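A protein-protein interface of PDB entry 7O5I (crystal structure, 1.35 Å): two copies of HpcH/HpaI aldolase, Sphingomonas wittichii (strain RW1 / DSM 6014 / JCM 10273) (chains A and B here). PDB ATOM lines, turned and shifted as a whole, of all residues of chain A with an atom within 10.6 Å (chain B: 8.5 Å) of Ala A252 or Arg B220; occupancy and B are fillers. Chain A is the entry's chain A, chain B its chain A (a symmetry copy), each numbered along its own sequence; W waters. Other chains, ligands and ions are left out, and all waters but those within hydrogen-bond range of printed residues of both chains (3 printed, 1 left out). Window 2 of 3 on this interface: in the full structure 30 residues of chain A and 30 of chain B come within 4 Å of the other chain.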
ATOM      1  N   ARG A 244      13.573 -14.691  28.397  1.00  0.00           N
ATOM      2  CA  ARG A 244      13.919 -13.347  28.840  1.00  0.00           C
ATOM      3  C   ARG A 244      13.249 -12.314  27.937  1.00  0.00           C
ATOM      4  O   ARG A 244      12.742 -11.294  28.406  1.00  0.00           O
ATOM      5  CB  ARG A 244      15.450 -13.212  28.874  1.00  0.00           C
ATOM      6  CG  ARG A 244      15.957 -11.898  29.373  1.00  0.00           C
ATOM      7  CD  ARG A 244      17.491 -11.925  29.353  1.00  0.00           C
ATOM      8  NE  ARG A 244      18.097 -12.689  30.444  1.00  0.00           N
ATOM      9  CZ  ARG A 244      18.194 -12.252  31.694  1.00  0.00           C
ATOM     10  NH1 ARG A 244      17.693 -11.080  32.058  1.00  0.00           N
ATOM     11  NH2 ARG A 244      18.812 -13.008  32.601  1.00  0.00           N
ATOM     12  N   GLN A 245      13.166 -12.601  26.656  1.00  0.00           N
ATOM     13  CA  GLN A 245      12.550 -11.665  25.737  1.00  0.00           C
ATOM     14  C   GLN A 245      11.042 -11.656  25.879  1.00  0.00           C
ATOM     15  O   GLN A 245      10.422 -10.603  25.740  1.00  0.00           O
ATOM     16  CB  GLN A 245      12.965 -11.962  24.300  1.00  0.00           C
ATOM     17  CG  GLN A 245      12.477 -10.915  23.318  1.00  0.00           C
ATOM     18  CD  GLN A 245      13.149  -9.574  23.583  1.00  0.00           C
ATOM     19  OE1 GLN A 245      14.377  -9.479  23.561  1.00  0.00           O
ATOM     20  NE2 GLN A 245      12.354  -8.529  23.814  1.00  0.00           N
ATOM     21  N   VAL A 246      10.435 -12.812  26.114  1.00  0.00           N
ATOM     22  CA  VAL A 246       8.991 -12.852  26.346  1.00  0.00           C
ATOM     23  C   VAL A 246       8.628 -12.050  27.572  1.00  0.00           C
ATOM     24  O   VAL A 246       7.661 -11.277  27.544  1.00  0.00           O
ATOM     25  CB  VAL A 246       8.500 -14.303  26.446  1.00  0.00           C
ATOM     26  CG1 VAL A 246       7.089 -14.350  27.053  1.00  0.00           C
ATOM     27  CG2 VAL A 246       8.467 -14.969  25.055  1.00  0.00           C
ATOM     28  N   ILE A 247       9.415 -12.177  28.644  1.00  0.00           N
ATOM     29  CA  ILE A 247       9.196 -11.410  29.869  1.00  0.00           C
ATOM     30  C   ILE A 247       9.332  -9.921  29.588  1.00  0.00           C
ATOM     31  O   ILE A 247       8.483  -9.122  30.001  1.00  0.00           O
ATOM     32  CB  ILE A 247      10.158 -11.889  30.974  1.00  0.00           C
ATOM     33  CG1 ILE A 247       9.829 -13.337  31.358  1.00  0.00           C
ATOM     34  CG2 ILE A 247      10.135 -10.957  32.160  1.00  0.00           C
ATOM     35  CD1 ILE A 247      10.886 -13.964  32.261  1.00  0.00           C
ATOM     36  N   ALA A 248      10.372  -9.527  28.846  1.00  0.00           N
ATOM     37  CA  ALA A 248      10.578  -8.105  28.566  1.00  0.00           C
ATOM     38  C   ALA A 248       9.418  -7.544  27.767  1.00  0.00           C
ATOM     39  O   ALA A 248       8.893  -6.455  28.083  1.00  0.00           O
ATOM     40  CB  ALA A 248      11.894  -7.902  27.801  1.00  0.00           C
ATOM     41  N   ASP A 249       8.943  -8.315  26.791  1.00  0.00           N
ATOM     42  CA  ASP A 249       7.806  -7.902  25.979  1.00  0.00           C
ATOM     43  C   ASP A 249       6.521  -7.840  26.809  1.00  0.00           C
ATOM     44  O   ASP A 249       5.709  -6.912  26.658  1.00  0.00           O
ATOM     45  CB  ASP A 249       7.627  -8.876  24.820  1.00  0.00           C
ATOM     46  CG  ASP A 249       8.741  -8.786  23.807  1.00  0.00           C
ATOM     47  OD1 ASP A 249       9.531  -7.829  23.867  1.00  0.00           O
ATOM     48  OD2 ASP A 249       8.808  -9.669  22.923  1.00  0.00           O
ATOM     49  N   ALA A 250       6.329  -8.804  27.706  1.00  0.00           N
ATOM     50  CA  ALA A 250       5.102  -8.848  28.493  1.00  0.00           C
ATOM     51  C   ALA A 250       5.058  -7.706  29.493  1.00  0.00           C
ATOM     52  O   ALA A 250       3.976  -7.170  29.764  1.00  0.00           O
ATOM     53  CB  ALA A 250       4.996 -10.190  29.234  1.00  0.00           C
ATOM     54  N   ARG A 251       6.214  -7.364  30.094  1.00  0.00           N
ATOM     55  CA  ARG A 251       6.299  -6.375  31.167  1.00  0.00           C
ATOM     56  C   ARG A 251       6.514  -4.961  30.661  1.00  0.00           C
ATOM     57  O   ARG A 251       6.481  -4.020  31.464  1.00  0.00           O
ATOM     58  CB  ARG A 251       7.404  -6.742  32.143  1.00  0.00           C
ATOM     59  CG  ARG A 251       7.161  -8.033  32.910  1.00  0.00           C
ATOM     60  CD  ARG A 251       8.064  -8.118  34.113  1.00  0.00           C
ATOM     61  NE  ARG A 251       7.854  -9.315  34.921  1.00  0.00           N
ATOM     62  CZ  ARG A 251       6.923  -9.445  35.860  1.00  0.00           C
ATOM     63  NH1 ARG A 251       5.996  -8.528  36.054  1.00  0.00           N
ATOM     64  NH2 ARG A 251       6.956 -10.490  36.671  1.00  0.00           N
ATOM     65  N   ALA A 252       6.726  -4.792  29.363  1.00  0.00           N
ATOM     66  CA  ALA A 252       6.888  -3.460  28.823  1.00  0.00           C
ATOM     67  C   ALA A 252       5.612  -2.659  29.009  1.00  0.00           C
ATOM     68  O   ALA A 252       4.509  -3.196  28.936  1.00  0.00           O
ATOM     69  CB  ALA A 252       7.211  -3.532  27.340  1.00  0.00           C
ATOM     70  N   LEU A 253       5.779  -1.361  29.227  1.00  0.00           N
ATOM     71  CA  LEU A 253       4.671  -0.409  29.180  1.00  0.00           C
ATOM     72  C   LEU A 253       4.048  -0.459  27.786  1.00  0.00           C
ATOM     73  O   LEU A 253       4.767  -0.648  26.793  1.00  0.00           O
ATOM     74  CB  LEU A 253       5.226   0.988  29.426  1.00  0.00           C
ATOM     75  CG  LEU A 253       5.694   1.270  30.849  1.00  0.00           C
ATOM     76  CD1 LEU A 253       6.178   2.711  30.983  1.00  0.00           C
ATOM     77  CD2 LEU A 253       4.571   1.000  31.837  1.00  0.00           C
ATOM     78  OXT LEU A 253       2.831  -0.361  27.604  1.00  0.00           O
ATOM     79  N   PRO B  15      -0.270  -7.467  39.096  1.00  0.00           N
ATOM     80  CA  PRO B  15      -0.506  -8.824  38.596  1.00  0.00           C
ATOM     81  C   PRO B  15       0.767  -9.654  38.681  1.00  0.00           C
ATOM     82  O   PRO B  15       1.840  -9.165  39.026  1.00  0.00           O
ATOM     83  CB  PRO B  15      -0.897  -8.583  37.136  1.00  0.00           C
ATOM     84  CG  PRO B  15      -0.106  -7.344  36.776  1.00  0.00           C
ATOM     85  CD  PRO B  15      -0.228  -6.473  38.009  1.00  0.00           C
ATOM     86  N   LEU B  17       3.169 -12.557  36.546  1.00  0.00           N
ATOM     87  CA  LEU B  17       3.559 -13.141  35.271  1.00  0.00           C
ATOM     88  C   LEU B  17       4.295 -14.443  35.553  1.00  0.00           C
ATOM     89  O   LEU B  17       5.190 -14.482  36.406  1.00  0.00           O
ATOM     90  CB  LEU B  17       4.513 -12.202  34.537  1.00  0.00           C
ATOM     91  CG  LEU B  17       4.987 -12.697  33.168  1.00  0.00           C
ATOM     92  CD1 LEU B  17       3.878 -12.683  32.151  1.00  0.00           C
ATOM     93  CD2 LEU B  17       6.179 -11.879  32.690  1.00  0.00           C
ATOM     94  N   CYS B 213      -1.104 -17.570  27.713  1.00  0.00           N
ATOM     95  CA  CYS B 213      -0.696 -16.814  26.535  1.00  0.00           C
ATOM     96  C   CYS B 213       0.459 -17.499  25.806  1.00  0.00           C
ATOM     97  O   CYS B 213       1.299 -18.190  26.401  1.00  0.00           O
ATOM     98  CB  CYS B 213      -0.243 -15.389  26.923  1.00  0.00           C
ATOM     99  SG  CYS B 213      -1.480 -14.481  27.848  1.00  0.00           S
ATOM    100  N   SER B 215       2.583 -15.668  23.674  1.00  0.00           N
ATOM    101  CA  SER B 215       3.534 -14.676  23.199  1.00  0.00           C
ATOM    102  C   SER B 215       3.619 -13.563  24.218  1.00  0.00           C
ATOM    103  O   SER B 215       2.660 -13.301  24.955  1.00  0.00           O
ATOM    104  CB  SER B 215       3.118 -14.109  21.833  1.00  0.00           C
ATOM    105  OG  SER B 215       1.897 -13.413  21.923  1.00  0.00           O
ATOM    106  N   GLY B 216       4.749 -12.856  24.179  1.00  0.00           N
ATOM    107  CA  GLY B 216       4.943 -11.741  25.087  1.00  0.00           C
ATOM    108  C   GLY B 216       4.029 -10.564  24.787  1.00  0.00           C
ATOM    109  O   GLY B 216       3.527  -9.907  25.700  1.00  0.00           O
ATOM    110  N   GLY B 217       3.810 -10.282  23.505  1.00  0.00           N
ATOM    111  CA  GLY B 217       2.947  -9.172  23.135  1.00  0.00           C
ATOM    112  C   GLY B 217       1.507  -9.405  23.558  1.00  0.00           C
ATOM    113  O   GLY B 217       0.827  -8.486  24.036  1.00  0.00           O
ATOM    114  N   PHE B 218       1.000 -10.626  23.352  1.00  0.00           N
ATOM    115  CA  PHE B 218      -0.363 -10.917  23.805  1.00  0.00           C
ATOM    116  C   PHE B 218      -0.465 -10.803  25.319  1.00  0.00           C
ATOM    117  O   PHE B 218      -1.444 -10.248  25.850  1.00  0.00           O
ATOM    118  CB  PHE B 218      -0.813 -12.295  23.331  1.00  0.00           C
ATOM    119  CG  PHE B 218      -2.260 -12.612  23.599  1.00  0.00           C
ATOM    120  CD1 PHE B 218      -2.609 -13.390  24.698  1.00  0.00           C
ATOM    121  CD2 PHE B 218      -3.244 -12.243  22.709  1.00  0.00           C
ATOM    122  CE1 PHE B 218      -3.946 -13.729  24.946  1.00  0.00           C
ATOM    123  CE2 PHE B 218      -4.576 -12.596  22.928  1.00  0.00           C
ATOM    124  CZ  PHE B 218      -4.916 -13.348  24.048  1.00  0.00           C
ATOM    125  N   ALA B 219       0.537 -11.337  26.032  1.00  0.00           N
ATOM    126  CA  ALA B 219       0.583 -11.218  27.484  1.00  0.00           C
ATOM    127  C   ALA B 219       0.541  -9.757  27.918  1.00  0.00           C
ATOM    128  O   ALA B 219      -0.142  -9.428  28.894  1.00  0.00           O
ATOM    129  CB  ALA B 219       1.839 -11.912  28.017  1.00  0.00           C
ATOM    130  N   ARG B 220       1.325  -8.880  27.256  1.00  0.00           N
ATOM    131  CA  ARG B 220       1.293  -7.461  27.597  1.00  0.00           C
ATOM    132  C   ARG B 220      -0.131  -6.908  27.503  1.00  0.00           C
ATOM    133  O   ARG B 220      -0.599  -6.184  28.399  1.00  0.00           O
ATOM    134  CB  ARG B 220       2.220  -6.670  26.680  1.00  0.00           C
ATOM    135  CG  ARG B 220       2.248  -5.184  27.070  1.00  0.00           C
ATOM    136  CD  ARG B 220       3.197  -4.377  26.197  1.00  0.00           C
ATOM    137  NE  ARG B 220       2.910  -4.523  24.783  1.00  0.00           N
ATOM    138  CZ  ARG B 220       1.825  -4.092  24.168  1.00  0.00           C
ATOM    139  NH1 ARG B 220       0.890  -3.411  24.809  1.00  0.00           N
ATOM    140  NH2 ARG B 220       1.683  -4.326  22.869  1.00  0.00           N
ATOM    141  N   VAL B 221      -0.837  -7.231  26.418  1.00  0.00           N
ATOM    142  CA  VAL B 221      -2.206  -6.742  26.251  1.00  0.00           C
ATOM    143  C   VAL B 221      -3.122  -7.323  27.327  1.00  0.00           C
ATOM    144  O   VAL B 221      -3.935  -6.602  27.916  1.00  0.00           O
ATOM    145  CB  VAL B 221      -2.697  -7.048  24.826  1.00  0.00           C
ATOM    146  CG1 VAL B 221      -4.177  -6.691  24.708  1.00  0.00           C
ATOM    147  CG2 VAL B 221      -1.855  -6.264  23.784  1.00  0.00           C
ATOM    148  N   LYS B 222      -2.986  -8.623  27.636  1.00  0.00           N
ATOM    149  CA  LYS B 222      -3.808  -9.200  28.701  1.00  0.00           C
ATOM    150  C   LYS B 222      -3.559  -8.504  30.045  1.00  0.00           C
ATOM    151  O   LYS B 222      -4.502  -8.255  30.813  1.00  0.00           O
ATOM    152  CB  LYS B 222      -3.537 -10.696  28.838  1.00  0.00           C
ATOM    153  CG  LYS B 222      -3.911 -11.568  27.643  1.00  0.00           C
ATOM    154  CD  LYS B 222      -5.303 -11.318  27.020  1.00  0.00           C
ATOM    155  CE  LYS B 222      -5.244 -10.376  25.819  1.00  0.00           C
ATOM    156  NZ  LYS B 222      -6.579 -10.164  25.182  1.00  0.00           N
ATOM    157  N   LEU B 223      -2.305  -8.162  30.340  1.00  0.00           N
ATOM    158  CA  LEU B 223      -2.009  -7.430  31.563  1.00  0.00           C
ATOM    159  C   LEU B 223      -2.682  -6.061  31.530  1.00  0.00           C
ATOM    160  O   LEU B 223      -3.262  -5.610  32.528  1.00  0.00           O
ATOM    161  CB  LEU B 223      -0.499  -7.303  31.748  1.00  0.00           C
ATOM    162  CG  LEU B 223       0.214  -8.605  32.121  1.00  0.00           C
ATOM    163  CD1 LEU B 223       1.746  -8.420  32.034  1.00  0.00           C
ATOM    164  CD2 LEU B 223      -0.168  -9.062  33.526  1.00  0.00           C
ATOM    165  N   ALA B 224      -2.612  -5.388  30.381  1.00  0.00           N
ATOM    166  CA  ALA B 224      -3.263  -4.084  30.236  1.00  0.00           C
ATOM    167  C   ALA B 224      -4.778  -4.178  30.415  1.00  0.00           C
ATOM    168  O   ALA B 224      -5.402  -3.238  30.917  1.00  0.00           O
ATOM    169  CB  ALA B 224      -2.922  -3.462  28.878  1.00  0.00           C
ATOM    170  N   GLU B 225      -5.399  -5.279  29.974  1.00  0.00           N
ATOM    171  CA  GLU B 225      -6.834  -5.512  30.144  1.00  0.00           C
ATOM    172  C   GLU B 225      -7.217  -5.813  31.586  1.00  0.00           C
ATOM    173  O   GLU B 225      -8.417  -5.835  31.909  1.00  0.00           O
ATOM    174  CB  GLU B 225      -7.284  -6.634  29.208  1.00  0.00           C
ATOM    175  CG  GLU B 225      -7.256  -6.272  27.728  1.00  0.00           C
ATOM    176  CD  GLU B 225      -7.705  -7.404  26.838  1.00  0.00           C
ATOM    177  OE1 GLU B 225      -7.676  -8.568  27.289  1.00  0.00           O
ATOM    178  OE2 GLU B 225      -8.047  -7.124  25.662  1.00  0.00           O
ATOM    179  N   GLY B 226      -6.236  -6.059  32.446  1.00  0.00           N
ATOM    180  CA  GLY B 226      -6.484  -6.284  33.855  1.00  0.00           C
ATOM    181  C   GLY B 226      -6.404  -7.716  34.336  1.00  0.00           C
ATOM    182  O   GLY B 226      -6.754  -7.973  35.490  1.00  0.00           O
ATOM    183  N   PHE B 227      -5.936  -8.658  33.524  1.00  0.00           N
ATOM    184  CA  PHE B 227      -5.749 -10.011  34.029  1.00  0.00           C
ATOM    185  C   PHE B 227      -4.774 -10.019  35.199  1.00  0.00           C
ATOM    186  O   PHE B 227      -3.752  -9.326  35.203  1.00  0.00           O
ATOM    187  CB  PHE B 227      -5.284 -10.941  32.921  1.00  0.00           C
ATOM    188  CG  PHE B 227      -6.396 -11.330  31.989  1.00  0.00           C
ATOM    189  CD1 PHE B 227      -6.720 -10.555  30.890  1.00  0.00           C
ATOM    190  CD2 PHE B 227      -7.144 -12.476  32.228  1.00  0.00           C
ATOM    191  CE1 PHE B 227      -7.773 -10.930  30.052  1.00  0.00           C
ATOM    192  CE2 PHE B 227      -8.163 -12.859  31.373  1.00  0.00           C
ATOM    193  CZ  PHE B 227      -8.469 -12.071  30.298  1.00  0.00           C
ATOM    194  N   VAL B 230      -0.924 -14.057  34.316  1.00  0.00           N
ATOM    195  CA  VAL B 230      -0.712 -14.249  32.891  1.00  0.00           C
ATOM    196  C   VAL B 230       0.475 -15.186  32.744  1.00  0.00           C
ATOM    197  O   VAL B 230       1.501 -14.956  33.380  1.00  0.00           O
ATOM    198  CB  VAL B 230      -0.447 -12.883  32.229  1.00  0.00           C
ATOM    199  CG1 VAL B 230      -0.108 -13.048  30.767  1.00  0.00           C
ATOM    200  CG2 VAL B 230      -1.660 -11.974  32.429  1.00  0.00           C
ATOM    201  N   THR B 231       0.331 -16.240  31.946  1.00  0.00           N
ATOM    202  CA  THR B 231       1.442 -17.131  31.641  1.00  0.00           C
ATOM    203  C   THR B 231       1.922 -16.874  30.225  1.00  0.00           C
ATOM    204  O   THR B 231       1.103 -16.706  29.311  1.00  0.00           O
ATOM    205  CB  THR B 231       1.063 -18.603  31.860  1.00  0.00           C
ATOM    206  OG1 THR B 231       0.137 -19.047  30.884  1.00  0.00           O
ATOM    207  CG2 THR B 231       0.501 -18.817  33.254  1.00  0.00           C
ATOM    208  N   ALA B 232       3.251 -16.880  30.049  1.00  0.00           N
ATOM    209  CA  ALA B 232       3.809 -16.708  28.711  1.00  0.00           C
ATOM    210  C   ALA B 232       5.271 -17.138  28.757  1.00  0.00           C
ATOM    211  O   ALA B 232       5.995 -16.664  29.644  1.00  0.00           O
ATOM    212  CB  ALA B 232       3.757 -15.241  28.268  1.00  0.00           C
HETATM  213  O   HOH W   1       4.227  -8.265  38.293  1.00  0.00           O
HETATM  214  O   HOH W   2       5.513  -5.744  24.171  1.00  0.00           O
HETATM  215  O   HOH W   3       0.784  -2.203  27.658  1.00  0.00           O
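Printed residues of chain A that touch a printed residue of chain B: Val A246, Asp A249, Ala A250, Arg A251 and Ala A252.
Hydrophobic or aromatic side chains of chain A within 4 Å of the printed part of chain B: Val A246 and Ala A250.
Along chain A the printed residues that touch a printed residue of chain B span positions 246 to 252.
Of the 19 printed residues of chain B, 6 touch a printed residue of chain A.
Printed residues of chain B that touch a printed residue of chain A: Leu B17, Gly B216, Ala B219, Arg B220, Leu B223 and Ala B232.
Water W1 bridges O of Pro B15 (2.7 Å) and NH1 of Arg A251 (2.9 Å).
Water W2 lies within hydrogen-bond range of the backbone carbonyl oxygen of Asp A249 (2.8 Å) and the guanidinium group of Arg B220 (2.9 Å).
Water W3 lies within hydrogen-bond range of OXT of Leu A253 (2.8 Å) and NH1 of Arg B220 (3.1 Å).
No position is printed for both chains.
Of the 11 pairs that touch across the chains among the printed residues, none has its exchanged pair printed and touching as well.
Printed residues of chain B within 4 Å of Val A246: Gly B216 (3.7 Å) and Ala B232 (3.6 Å).
Printed residues of chain B within 4 Å of Arg A251: Leu B17 (3.7 Å).
Of chain B, only Arg B220 (3.3 Å) comes within 4 Å of Ala A252.
Of chain A, only Val A246 (3.7 Å), Asp A249 (3.8 Å) and Ala A250 (3.4 Å) come within 4 Å of Gly B216.
No residue of chain A comes within 4 Å of Gly B217.
Ala B219 touches one residue of chain A.
Of chain A, only Asp A249, Ala A250 and Ala A252 come within 4 Å of Arg B220.
Of chain A, only Ala A250 comes within 4 Å of Leu B223.
No residue of chain A comes within 4 Å of Ala B224.
Printed residues of chain A within 4 Å of Ala B232: Val A246.
The nearest residue of chain B that does not touch Ala A252 is Leu B223 (6.7 Å).
The nearest residue of chain A that does not touch Arg B220 is Leu A253 (4.1 Å).
The nearest printed residue of chain B that does not touch Asp A249 is Gly B217 (4.3 Å).
Val A246 touches Gly B216.
Val A246 touches Ala B232 (CG1 to O, 3.6 Å).
Gly B216 touches Asp A249 (O to C, 3.8 Å).
O of Asp A249 touches CB of Arg B220, at 3.5 Å.
Ala A250 touches Leu B17.
CB of Ala A250 touches CB of Ala B219, 3.8 Å away.
O of Ala A250 touches CA of Arg B220, at 3.5 Å.
Leu B223 touches Ala A250.
Arg A251 touches Leu B17.
O of Ala A252 touches CD of Arg B220, at 3.3 Å.
The side-chain amide nitrogen of Gln A245 is in hydrogen-bond range of the side-chain carboxylate of Asp A249, at 2.9 Å.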
